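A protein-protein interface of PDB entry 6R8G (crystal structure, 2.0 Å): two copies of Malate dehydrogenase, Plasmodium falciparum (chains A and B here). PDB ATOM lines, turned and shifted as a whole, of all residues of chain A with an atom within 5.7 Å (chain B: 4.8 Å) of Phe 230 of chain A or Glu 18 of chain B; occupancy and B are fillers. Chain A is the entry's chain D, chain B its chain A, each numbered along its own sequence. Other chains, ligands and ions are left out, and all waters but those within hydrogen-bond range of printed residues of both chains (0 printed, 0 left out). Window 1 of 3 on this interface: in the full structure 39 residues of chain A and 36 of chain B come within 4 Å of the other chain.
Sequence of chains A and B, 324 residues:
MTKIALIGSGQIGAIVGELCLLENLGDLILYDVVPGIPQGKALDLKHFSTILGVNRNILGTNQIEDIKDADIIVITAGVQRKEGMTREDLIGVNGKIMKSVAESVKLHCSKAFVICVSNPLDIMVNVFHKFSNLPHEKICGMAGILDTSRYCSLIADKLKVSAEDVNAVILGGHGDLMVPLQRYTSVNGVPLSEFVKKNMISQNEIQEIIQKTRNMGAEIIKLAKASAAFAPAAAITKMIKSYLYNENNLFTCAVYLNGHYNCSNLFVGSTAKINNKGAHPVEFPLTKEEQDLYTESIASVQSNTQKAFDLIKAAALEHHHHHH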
ATOM      1  N   GLN A  11     -19.723  -5.978  -3.753  1.00  0.00           N
ATOM      2  CA  GLN A  11     -20.437  -6.566  -2.599  1.00  0.00           C
ATOM      3  C   GLN A  11     -20.166  -8.067  -2.514  1.00  0.00           C
ATOM      4  O   GLN A  11     -19.844  -8.537  -1.424  1.00  0.00           O
ATOM      5  CB  GLN A  11     -21.960  -6.308  -2.594  1.00  0.00           C
ATOM      6  CG  GLN A  11     -22.396  -5.039  -1.847  1.00  0.00           C
ATOM      7  CD  GLN A  11     -22.002  -5.084  -0.385  1.00  0.00           C
ATOM      8  OE1 GLN A  11     -20.900  -4.748   0.017  1.00  0.00           O
ATOM      9  NE2 GLN A  11     -22.882  -5.582   0.433  1.00  0.00           N
ATOM     10  N   ILE A  15     -17.678 -10.157   0.295  1.00  0.00           N
ATOM     11  CA  ILE A  15     -18.295 -11.105   1.248  1.00  0.00           C
ATOM     12  C   ILE A  15     -17.712 -12.512   1.050  1.00  0.00           C
ATOM     13  O   ILE A  15     -17.446 -13.202   2.067  1.00  0.00           O
ATOM     14  CB  ILE A  15     -19.822 -11.070   1.226  1.00  0.00           C
ATOM     15  CG1 ILE A  15     -20.354  -9.698   1.627  1.00  0.00           C
ATOM     16  CG2 ILE A  15     -20.344 -12.137   2.188  1.00  0.00           C
ATOM     17  CD1 ILE A  15     -21.785  -9.498   1.286  1.00  0.00           C
ATOM     18  N   GLU A  18     -14.490 -12.331   2.897  1.00  0.00           N
ATOM     19  CA  GLU A  18     -14.800 -12.411   4.345  1.00  0.00           C
ATOM     20  C   GLU A  18     -15.028 -13.882   4.754  1.00  0.00           C
ATOM     21  O   GLU A  18     -14.487 -14.296   5.759  1.00  0.00           O
ATOM     22  CB  GLU A  18     -16.025 -11.528   4.660  1.00  0.00           C
ATOM     23  CG  GLU A  18     -16.380 -11.543   6.149  1.00  0.00           C
ATOM     24  CD  GLU A  18     -17.869 -11.567   6.424  1.00  0.00           C
ATOM     25  OE1 GLU A  18     -18.611 -12.106   5.586  1.00  0.00           O
ATOM     26  OE2 GLU A  18     -18.288 -11.012   7.490  1.00  0.00           O
ATOM     27  N   LEU A  19     -15.876 -14.603   4.031  1.00  0.00           N
ATOM     28  CA  LEU A  19     -16.270 -15.985   4.385  1.00  0.00           C
ATOM     29  C   LEU A  19     -15.077 -16.904   4.158  1.00  0.00           C
ATOM     30  O   LEU A  19     -14.922 -17.808   4.997  1.00  0.00           O
ATOM     31  CB  LEU A  19     -17.473 -16.431   3.550  1.00  0.00           C
ATOM     32  CG  LEU A  19     -18.756 -15.629   3.777  1.00  0.00           C
ATOM     33  CD1 LEU A  19     -19.814 -16.088   2.809  1.00  0.00           C
ATOM     34  CD2 LEU A  19     -19.281 -15.771   5.206  1.00  0.00           C
ATOM     35  N   LEU A  22     -13.015 -16.364   7.382  1.00  0.00           N
ATOM     36  CA  LEU A  22     -13.678 -17.064   8.510  1.00  0.00           C
ATOM     37  C   LEU A  22     -13.453 -18.583   8.422  1.00  0.00           C
ATOM     38  O   LEU A  22     -13.245 -19.200   9.444  1.00  0.00           O
ATOM     39  CB  LEU A  22     -15.166 -16.747   8.505  1.00  0.00           C
ATOM     40  CG  LEU A  22     -15.493 -15.362   9.053  1.00  0.00           C
ATOM     41  CD1 LEU A  22     -16.935 -14.960   8.738  1.00  0.00           C
ATOM     42  CD2 LEU A  22     -15.192 -15.274  10.557  1.00  0.00           C
ATOM     43  N   ALA A 228     -29.082  -9.637  -4.236  1.00  0.00           N
ATOM     44  CA  ALA A 228     -28.624 -10.546  -3.178  1.00  0.00           C
ATOM     45  C   ALA A 228     -27.070 -10.538  -3.160  1.00  0.00           C
ATOM     46  O   ALA A 228     -26.442 -10.536  -4.224  1.00  0.00           O
ATOM     47  CB  ALA A 228     -29.267 -11.867  -3.450  1.00  0.00           C
ATOM     48  N   ALA A 229     -26.447 -10.579  -1.989  1.00  0.00           N
ATOM     49  CA  ALA A 229     -24.978 -10.620  -1.858  1.00  0.00           C
ATOM     50  C   ALA A 229     -24.549 -11.698  -0.854  1.00  0.00           C
ATOM     51  O   ALA A 229     -23.652 -12.472  -1.163  1.00  0.00           O
ATOM     52  CB  ALA A 229     -24.491  -9.235  -1.519  1.00  0.00           C
ATOM     53  N   PHE A 230     -25.160 -11.782   0.317  1.00  0.00           N
ATOM     54  CA  PHE A 230     -24.767 -12.749   1.385  1.00  0.00           C
ATOM     55  C   PHE A 230     -24.944 -14.185   0.899  1.00  0.00           C
ATOM     56  O   PHE A 230     -24.018 -14.988   1.042  1.00  0.00           O
ATOM     57  CB  PHE A 230     -25.494 -12.475   2.710  1.00  0.00           C
ATOM     58  CG  PHE A 230     -25.039 -11.202   3.390  1.00  0.00           C
ATOM     59  CD1 PHE A 230     -23.848 -11.177   4.094  1.00  0.00           C
ATOM     60  CD2 PHE A 230     -25.783 -10.034   3.319  1.00  0.00           C
ATOM     61  CE1 PHE A 230     -23.424 -10.027   4.733  1.00  0.00           C
ATOM     62  CE2 PHE A 230     -25.301  -8.863   3.902  1.00  0.00           C
ATOM     63  CZ  PHE A 230     -24.146  -8.867   4.636  1.00  0.00           C
ATOM     64  N   ALA A 231     -26.121 -14.530   0.370  1.00  0.00           N
ATOM     65  CA  ALA A 231     -26.411 -15.932  -0.020  1.00  0.00           C
ATOM     66  C   ALA A 231     -25.555 -16.334  -1.211  1.00  0.00           C
ATOM     67  O   ALA A 231     -24.959 -17.410  -1.222  1.00  0.00           O
ATOM     68  CB  ALA A 231     -27.881 -16.063  -0.254  1.00  0.00           C
ATOM     69  N   PRO A 232     -25.422 -15.513  -2.275  1.00  0.00           N
ATOM     70  CA  PRO A 232     -24.497 -15.826  -3.358  1.00  0.00           C
ATOM     71  C   PRO A 232     -23.071 -16.099  -2.851  1.00  0.00           C
ATOM     72  O   PRO A 232     -22.456 -17.043  -3.277  1.00  0.00           O
ATOM     73  CB  PRO A 232     -24.555 -14.592  -4.271  1.00  0.00           C
ATOM     74  CG  PRO A 232     -25.881 -13.978  -3.995  1.00  0.00           C
ATOM     75  CD  PRO A 232     -26.200 -14.295  -2.547  1.00  0.00           C
ATOM     76  N   ALA A 233     -22.576 -15.279  -1.924  1.00  0.00           N
ATOM     77  CA  ALA A 233     -21.232 -15.425  -1.346  1.00  0.00           C
ATOM     78  C   ALA A 233     -21.150 -16.763  -0.620  1.00  0.00           C
ATOM     79  O   ALA A 233     -20.123 -17.416  -0.779  1.00  0.00           O
ATOM     80  CB  ALA A 233     -20.926 -14.258  -0.423  1.00  0.00           C
ATOM     81  N   ALA A 234     -22.157 -17.123   0.189  1.00  0.00           N
ATOM     82  CA  ALA A 234     -22.145 -18.405   0.911  1.00  0.00           C
ATOM     83  C   ALA A 234     -22.079 -19.552  -0.110  1.00  0.00           C
ATOM     84  O   ALA A 234     -21.329 -20.510   0.113  1.00  0.00           O
ATOM     85  CB  ALA A 234     -23.357 -18.519   1.792  1.00  0.00           C
ATOM     86  N   ALA A 235     -22.840 -19.466  -1.211  1.00  0.00           N
ATOM     87  CA  ALA A 235     -22.901 -20.554  -2.224  1.00  0.00           C
ATOM     88  C   ALA A 235     -21.523 -20.704  -2.850  1.00  0.00           C
ATOM     89  O   ALA A 235     -21.019 -21.847  -2.977  1.00  0.00           O
ATOM     90  CB  ALA A 235     -23.934 -20.243  -3.280  1.00  0.00           C
ATOM     91  N   ALA B  14     -25.940  -4.980   8.752  1.00  0.00           N
ATOM     92  CA  ALA B  14     -26.194  -6.260   8.040  1.00  0.00           C
ATOM     93  C   ALA B  14     -25.067  -7.231   8.363  1.00  0.00           C
ATOM     94  O   ALA B  14     -25.356  -8.420   8.557  1.00  0.00           O
ATOM     95  CB  ALA B  14     -26.349  -6.067   6.564  1.00  0.00           C
ATOM     96  N   ILE B  15     -23.836  -6.745   8.407  1.00  0.00           N
ATOM     97  CA  ILE B  15     -22.670  -7.629   8.683  1.00  0.00           C
ATOM     98  C   ILE B  15     -22.677  -8.058  10.146  1.00  0.00           C
ATOM     99  O   ILE B  15     -22.365  -9.222  10.413  1.00  0.00           O
ATOM    100  CB  ILE B  15     -21.337  -7.004   8.244  1.00  0.00           C
ATOM    101  CG1 ILE B  15     -21.305  -6.748   6.732  1.00  0.00           C
ATOM    102  CG2 ILE B  15     -20.202  -7.905   8.663  1.00  0.00           C
ATOM    103  CD1 ILE B  15     -20.241  -5.799   6.325  1.00  0.00           C
ATOM    104  N   VAL B  16     -23.099  -7.214  11.064  1.00  0.00           N
ATOM    105  CA  VAL B  16     -23.334  -7.630  12.475  1.00  0.00           C
ATOM    106  C   VAL B  16     -24.374  -8.739  12.497  1.00  0.00           C
ATOM    107  O   VAL B  16     -24.122  -9.774  13.125  1.00  0.00           O
ATOM    108  CB  VAL B  16     -23.707  -6.459  13.380  1.00  0.00           C
ATOM    109  CG1 VAL B  16     -24.142  -6.968  14.724  1.00  0.00           C
ATOM    110  CG2 VAL B  16     -22.576  -5.458  13.521  1.00  0.00           C
ATOM    111  N   GLY B  17     -25.462  -8.582  11.778  1.00  0.00           N
ATOM    112  CA  GLY B  17     -26.455  -9.661  11.666  1.00  0.00           C
ATOM    113  C   GLY B  17     -25.832 -10.955  11.161  1.00  0.00           C
ATOM    114  O   GLY B  17     -26.057 -12.042  11.763  1.00  0.00           O
ATOM    115  N   GLU B  18     -25.084 -10.859  10.055  1.00  0.00           N
ATOM    116  CA  GLU B  18     -24.382 -12.015   9.439  1.00  0.00           C
ATOM    117  C   GLU B  18     -23.499 -12.730  10.483  1.00  0.00           C
ATOM    118  O   GLU B  18     -23.599 -13.925  10.597  1.00  0.00           O
ATOM    119  CB  GLU B  18     -23.578 -11.538   8.241  1.00  0.00           C
ATOM    120  CG  GLU B  18     -22.899 -12.662   7.501  1.00  0.00           C
ATOM    121  CD  GLU B  18     -21.514 -12.299   7.000  1.00  0.00           C
ATOM    122  OE1 GLU B  18     -20.799 -11.473   7.698  1.00  0.00           O
ATOM    123  OE2 GLU B  18     -21.136 -12.835   5.930  1.00  0.00           O
ATOM    124  N   LEU B  19     -22.687 -11.984  11.223  1.00  0.00           N
ATOM    125  CA  LEU B  19     -21.713 -12.537  12.190  1.00  0.00           C
ATOM    126  C   LEU B  19     -22.474 -13.099  13.370  1.00  0.00           C
ATOM    127  O   LEU B  19     -22.066 -14.160  13.816  1.00  0.00           O
ATOM    128  CB  LEU B  19     -20.718 -11.457  12.605  1.00  0.00           C
ATOM    129  CG  LEU B  19     -19.824 -10.925  11.488  1.00  0.00           C
ATOM    130  CD1 LEU B  19     -18.947  -9.799  11.978  1.00  0.00           C
ATOM    131  CD2 LEU B  19     -18.925 -11.998  10.919  1.00  0.00           C
ATOM    132  N   CYS B  20     -23.601 -12.484  13.806  1.00  0.00           N
ATOM    133  CA  CYS B  20     -24.427 -13.061  14.894  1.00  0.00           C
ATOM    134  C   CYS B  20     -25.053 -14.404  14.456  1.00  0.00           C
ATOM    135  O   CYS B  20     -25.115 -15.300  15.289  1.00  0.00           O
ATOM    136  CB  CYS B  20     -25.502 -12.082  15.345  1.00  0.00           C
ATOM    137  SG  CYS B  20     -24.807 -10.689  16.287  1.00  0.00           S
ATOM    138  N   LEU B  21     -25.458 -14.549  13.188  1.00  0.00           N
ATOM    139  CA  LEU B  21     -26.008 -15.808  12.636  1.00  0.00           C
ATOM    140  C   LEU B  21     -24.895 -16.870  12.591  1.00  0.00           C
ATOM    141  O   LEU B  21     -25.155 -17.963  13.051  1.00  0.00           O
ATOM    142  CB  LEU B  21     -26.628 -15.569  11.248  1.00  0.00           C
ATOM    143  CG  LEU B  21     -27.853 -14.671  11.248  1.00  0.00           C
ATOM    144  CD1 LEU B  21     -28.178 -14.136   9.846  1.00  0.00           C
ATOM    145  CD2 LEU B  21     -29.069 -15.399  11.845  1.00  0.00           C
ATOM    146  N   LEU B  22     -23.725 -16.544  12.065  1.00  0.00           N
ATOM    147  CA  LEU B  22     -22.602 -17.505  11.999  1.00  0.00           C
ATOM    148  C   LEU B  22     -22.223 -17.971  13.405  1.00  0.00           C
ATOM    149  O   LEU B  22     -21.894 -19.122  13.539  1.00  0.00           O
ATOM    150  CB  LEU B  22     -21.414 -16.830  11.325  1.00  0.00           C
ATOM    151  CG  LEU B  22     -21.539 -16.735   9.820  1.00  0.00           C
ATOM    152  CD1 LEU B  22     -20.459 -15.886   9.232  1.00  0.00           C
ATOM    153  CD2 LEU B  22     -21.473 -18.140   9.191  1.00  0.00           C
ATOM    154  N   ASP B  44     -32.156 -12.087   2.277  1.00  0.00           N
ATOM    155  CA  ASP B  44     -30.800 -12.496   1.871  1.00  0.00           C
ATOM    156  C   ASP B  44     -30.150 -13.301   3.009  1.00  0.00           C
ATOM    157  O   ASP B  44     -29.595 -14.377   2.771  1.00  0.00           O
ATOM    158  CB  ASP B  44     -30.008 -11.271   1.434  1.00  0.00           C
ATOM    159  CG  ASP B  44     -28.736 -11.608   0.662  1.00  0.00           C
ATOM    160  OD1 ASP B  44     -28.641 -12.761   0.131  1.00  0.00           O
ATOM    161  OD2 ASP B  44     -27.887 -10.721   0.628  1.00  0.00           O
ATOM    162  N   LEU B  45     -30.224 -12.799   4.237  1.00  0.00           N
ATOM    163  CA  LEU B  45     -29.566 -13.449   5.396  1.00  0.00           C
ATOM    164  C   LEU B  45     -30.289 -14.761   5.747  1.00  0.00           C
ATOM    165  O   LEU B  45     -29.572 -15.691   6.184  1.00  0.00           O
ATOM    166  CB  LEU B  45     -29.512 -12.437   6.543  1.00  0.00           C
ATOM    167  CG  LEU B  45     -28.512 -11.305   6.366  1.00  0.00           C
ATOM    168  CD1 LEU B  45     -28.670 -10.321   7.478  1.00  0.00           C
ATOM    169  CD2 LEU B  45     -27.074 -11.834   6.329  1.00  0.00           C
ATOM    170  N   PHE B  48     -28.775 -17.157   3.137  1.00  0.00           N
ATOM    171  CA  PHE B  48     -27.397 -17.355   3.605  1.00  0.00           C
ATOM    172  C   PHE B  48     -27.400 -18.390   4.748  1.00  0.00           C
ATOM    173  O   PHE B  48     -26.562 -19.339   4.740  1.00  0.00           O
ATOM    174  CB  PHE B  48     -26.878 -16.001   4.036  1.00  0.00           C
ATOM    175  CG  PHE B  48     -25.648 -16.000   4.893  1.00  0.00           C
ATOM    176  CD1 PHE B  48     -24.403 -15.898   4.317  1.00  0.00           C
ATOM    177  CD2 PHE B  48     -25.744 -16.016   6.279  1.00  0.00           C
ATOM    178  CE1 PHE B  48     -23.268 -15.809   5.115  1.00  0.00           C
ATOM    179  CE2 PHE B  48     -24.607 -16.000   7.069  1.00  0.00           C
ATOM    180  CZ  PHE B  48     -23.379 -15.894   6.488  1.00  0.00           C
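Of the 12 printed residues of chain B, 7 touch a printed residue of chain A.
Hydrophobic or aromatic side chains of chain B within 4 Å of the printed part of chain A: Ile 15, Leu 19, Leu 22, Leu 45 and Phe 48.
Hydrophobic or aromatic side chains of chain A that line the printed part of chain B: Ile 15, Leu 19, Leu 22, Ala 228, Phe 230, Ala 231, Pro 232 and Ala 234.
Ile 15 of chain A touches Glu 18 of chain B.
Glu 18 of chain A touches Ile 15 of chain B.
Glu 18 of chain A touches Leu 19 of chain B (OE2 to CD2, 3.6 Å).
Phe 48 of chain B touches Leu 19 of chain A.
Leu 22 of chain A touches Leu 22 of chain B (CD1 to CD1, 3.7 Å).
Ala 228 of chain A touches Asp 44 of chain B (CB to OD1, 3.7 Å).
Phe 230 of chain A touches Phe 48 of chain B (O to CD1, 3.4 Å).
N of Phe 48 of chain B touches CB of Ala 231 of chain A, 3.7 Å away.
Pro 232 of chain A touches Asp 44 of chain B (CD to OD1, 3.9 Å).
Phe 48 of chain B touches Ala 234 of chain A.
Printed residues of chain B within 4 Å of Phe 230 of chain A: Glu 18 (3.7 Å), Asp 44 (2.9 Å), Leu 45 (3.6 Å) and Phe 48 (3.4 Å).
Printed residues of chain A within 4 Å of Glu 18 of chain B: Ile 15, Glu 18, Leu 19 and Phe 230.
Printed residues of chain A within 4 Å of Leu 19 of chain B: Glu 18 (3.6 Å).
Of the printed residues of chain B, Pro 232 of chain A touches Asp 44.
Of the printed residues of chain B, Glu 18 of chain A touches Ile 15 (3.8 Å), Glu 18 (2.6 Å) and Leu 19 (3.6 Å).
Printed residues of chain A within 4 Å of Phe 48 of chain B: Leu 19 (3.99 Å), Phe 230 (3.4 Å), Ala 231 (3.7 Å) and Ala 234 (3.8 Å).
Leu 21 of chain B touches none of the printed residues of chain A.
The nearest printed residue of chain B that does not touch Phe 230 of chain A is Ala 14 of chain B (4.0003 Å).
The nearest residue of chain A that does not touch Glu 18 of chain B is Leu 22 of chain A (5.3 Å).
The nearest printed residue of chain B that does not touch Leu 22 of chain A is Leu 19 of chain B (4.2 Å).
The side-chain carboxylate (OE1) of Glu 18 of chain B lies close to the side-chain carboxylate (OE2) of Glu 18 of chain A, at 2.6 Å.
The side-chain carboxylate (OD2) of Asp 44 of chain B lies within hydrogen-bond range of the backbone NH (N) of Ala 229 of chain A (3.0 Å).
The side-chain carboxylate of Asp 44 of chain B sits at hydrogen-bond distance from the backbone NH of Ala 231 of chain A (3.1 Å).
The side-chain carboxylate (OD2) of Asp 44 of chain B sits at hydrogen-bond distance from the backbone NH (N) of Phe 230 of chain A.
Ile 15 of chain A touches Glu 18 of chain B, and with the chains exchanged Glu 18 of chain A touches Ile 15 of chain B.
Glu 18 of chain B touches its own counterpart, Glu 18 of chain A.
Glu 18 of chain A touches Leu 19 of chain B, and with the chains exchanged Leu 19 of chain A touches Glu 18 of chain B.
Leu 22 of chain A touches its own counterpart, Leu 22 of chain B.
Positions printed for both chains: 15, 18, 19 and 22.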
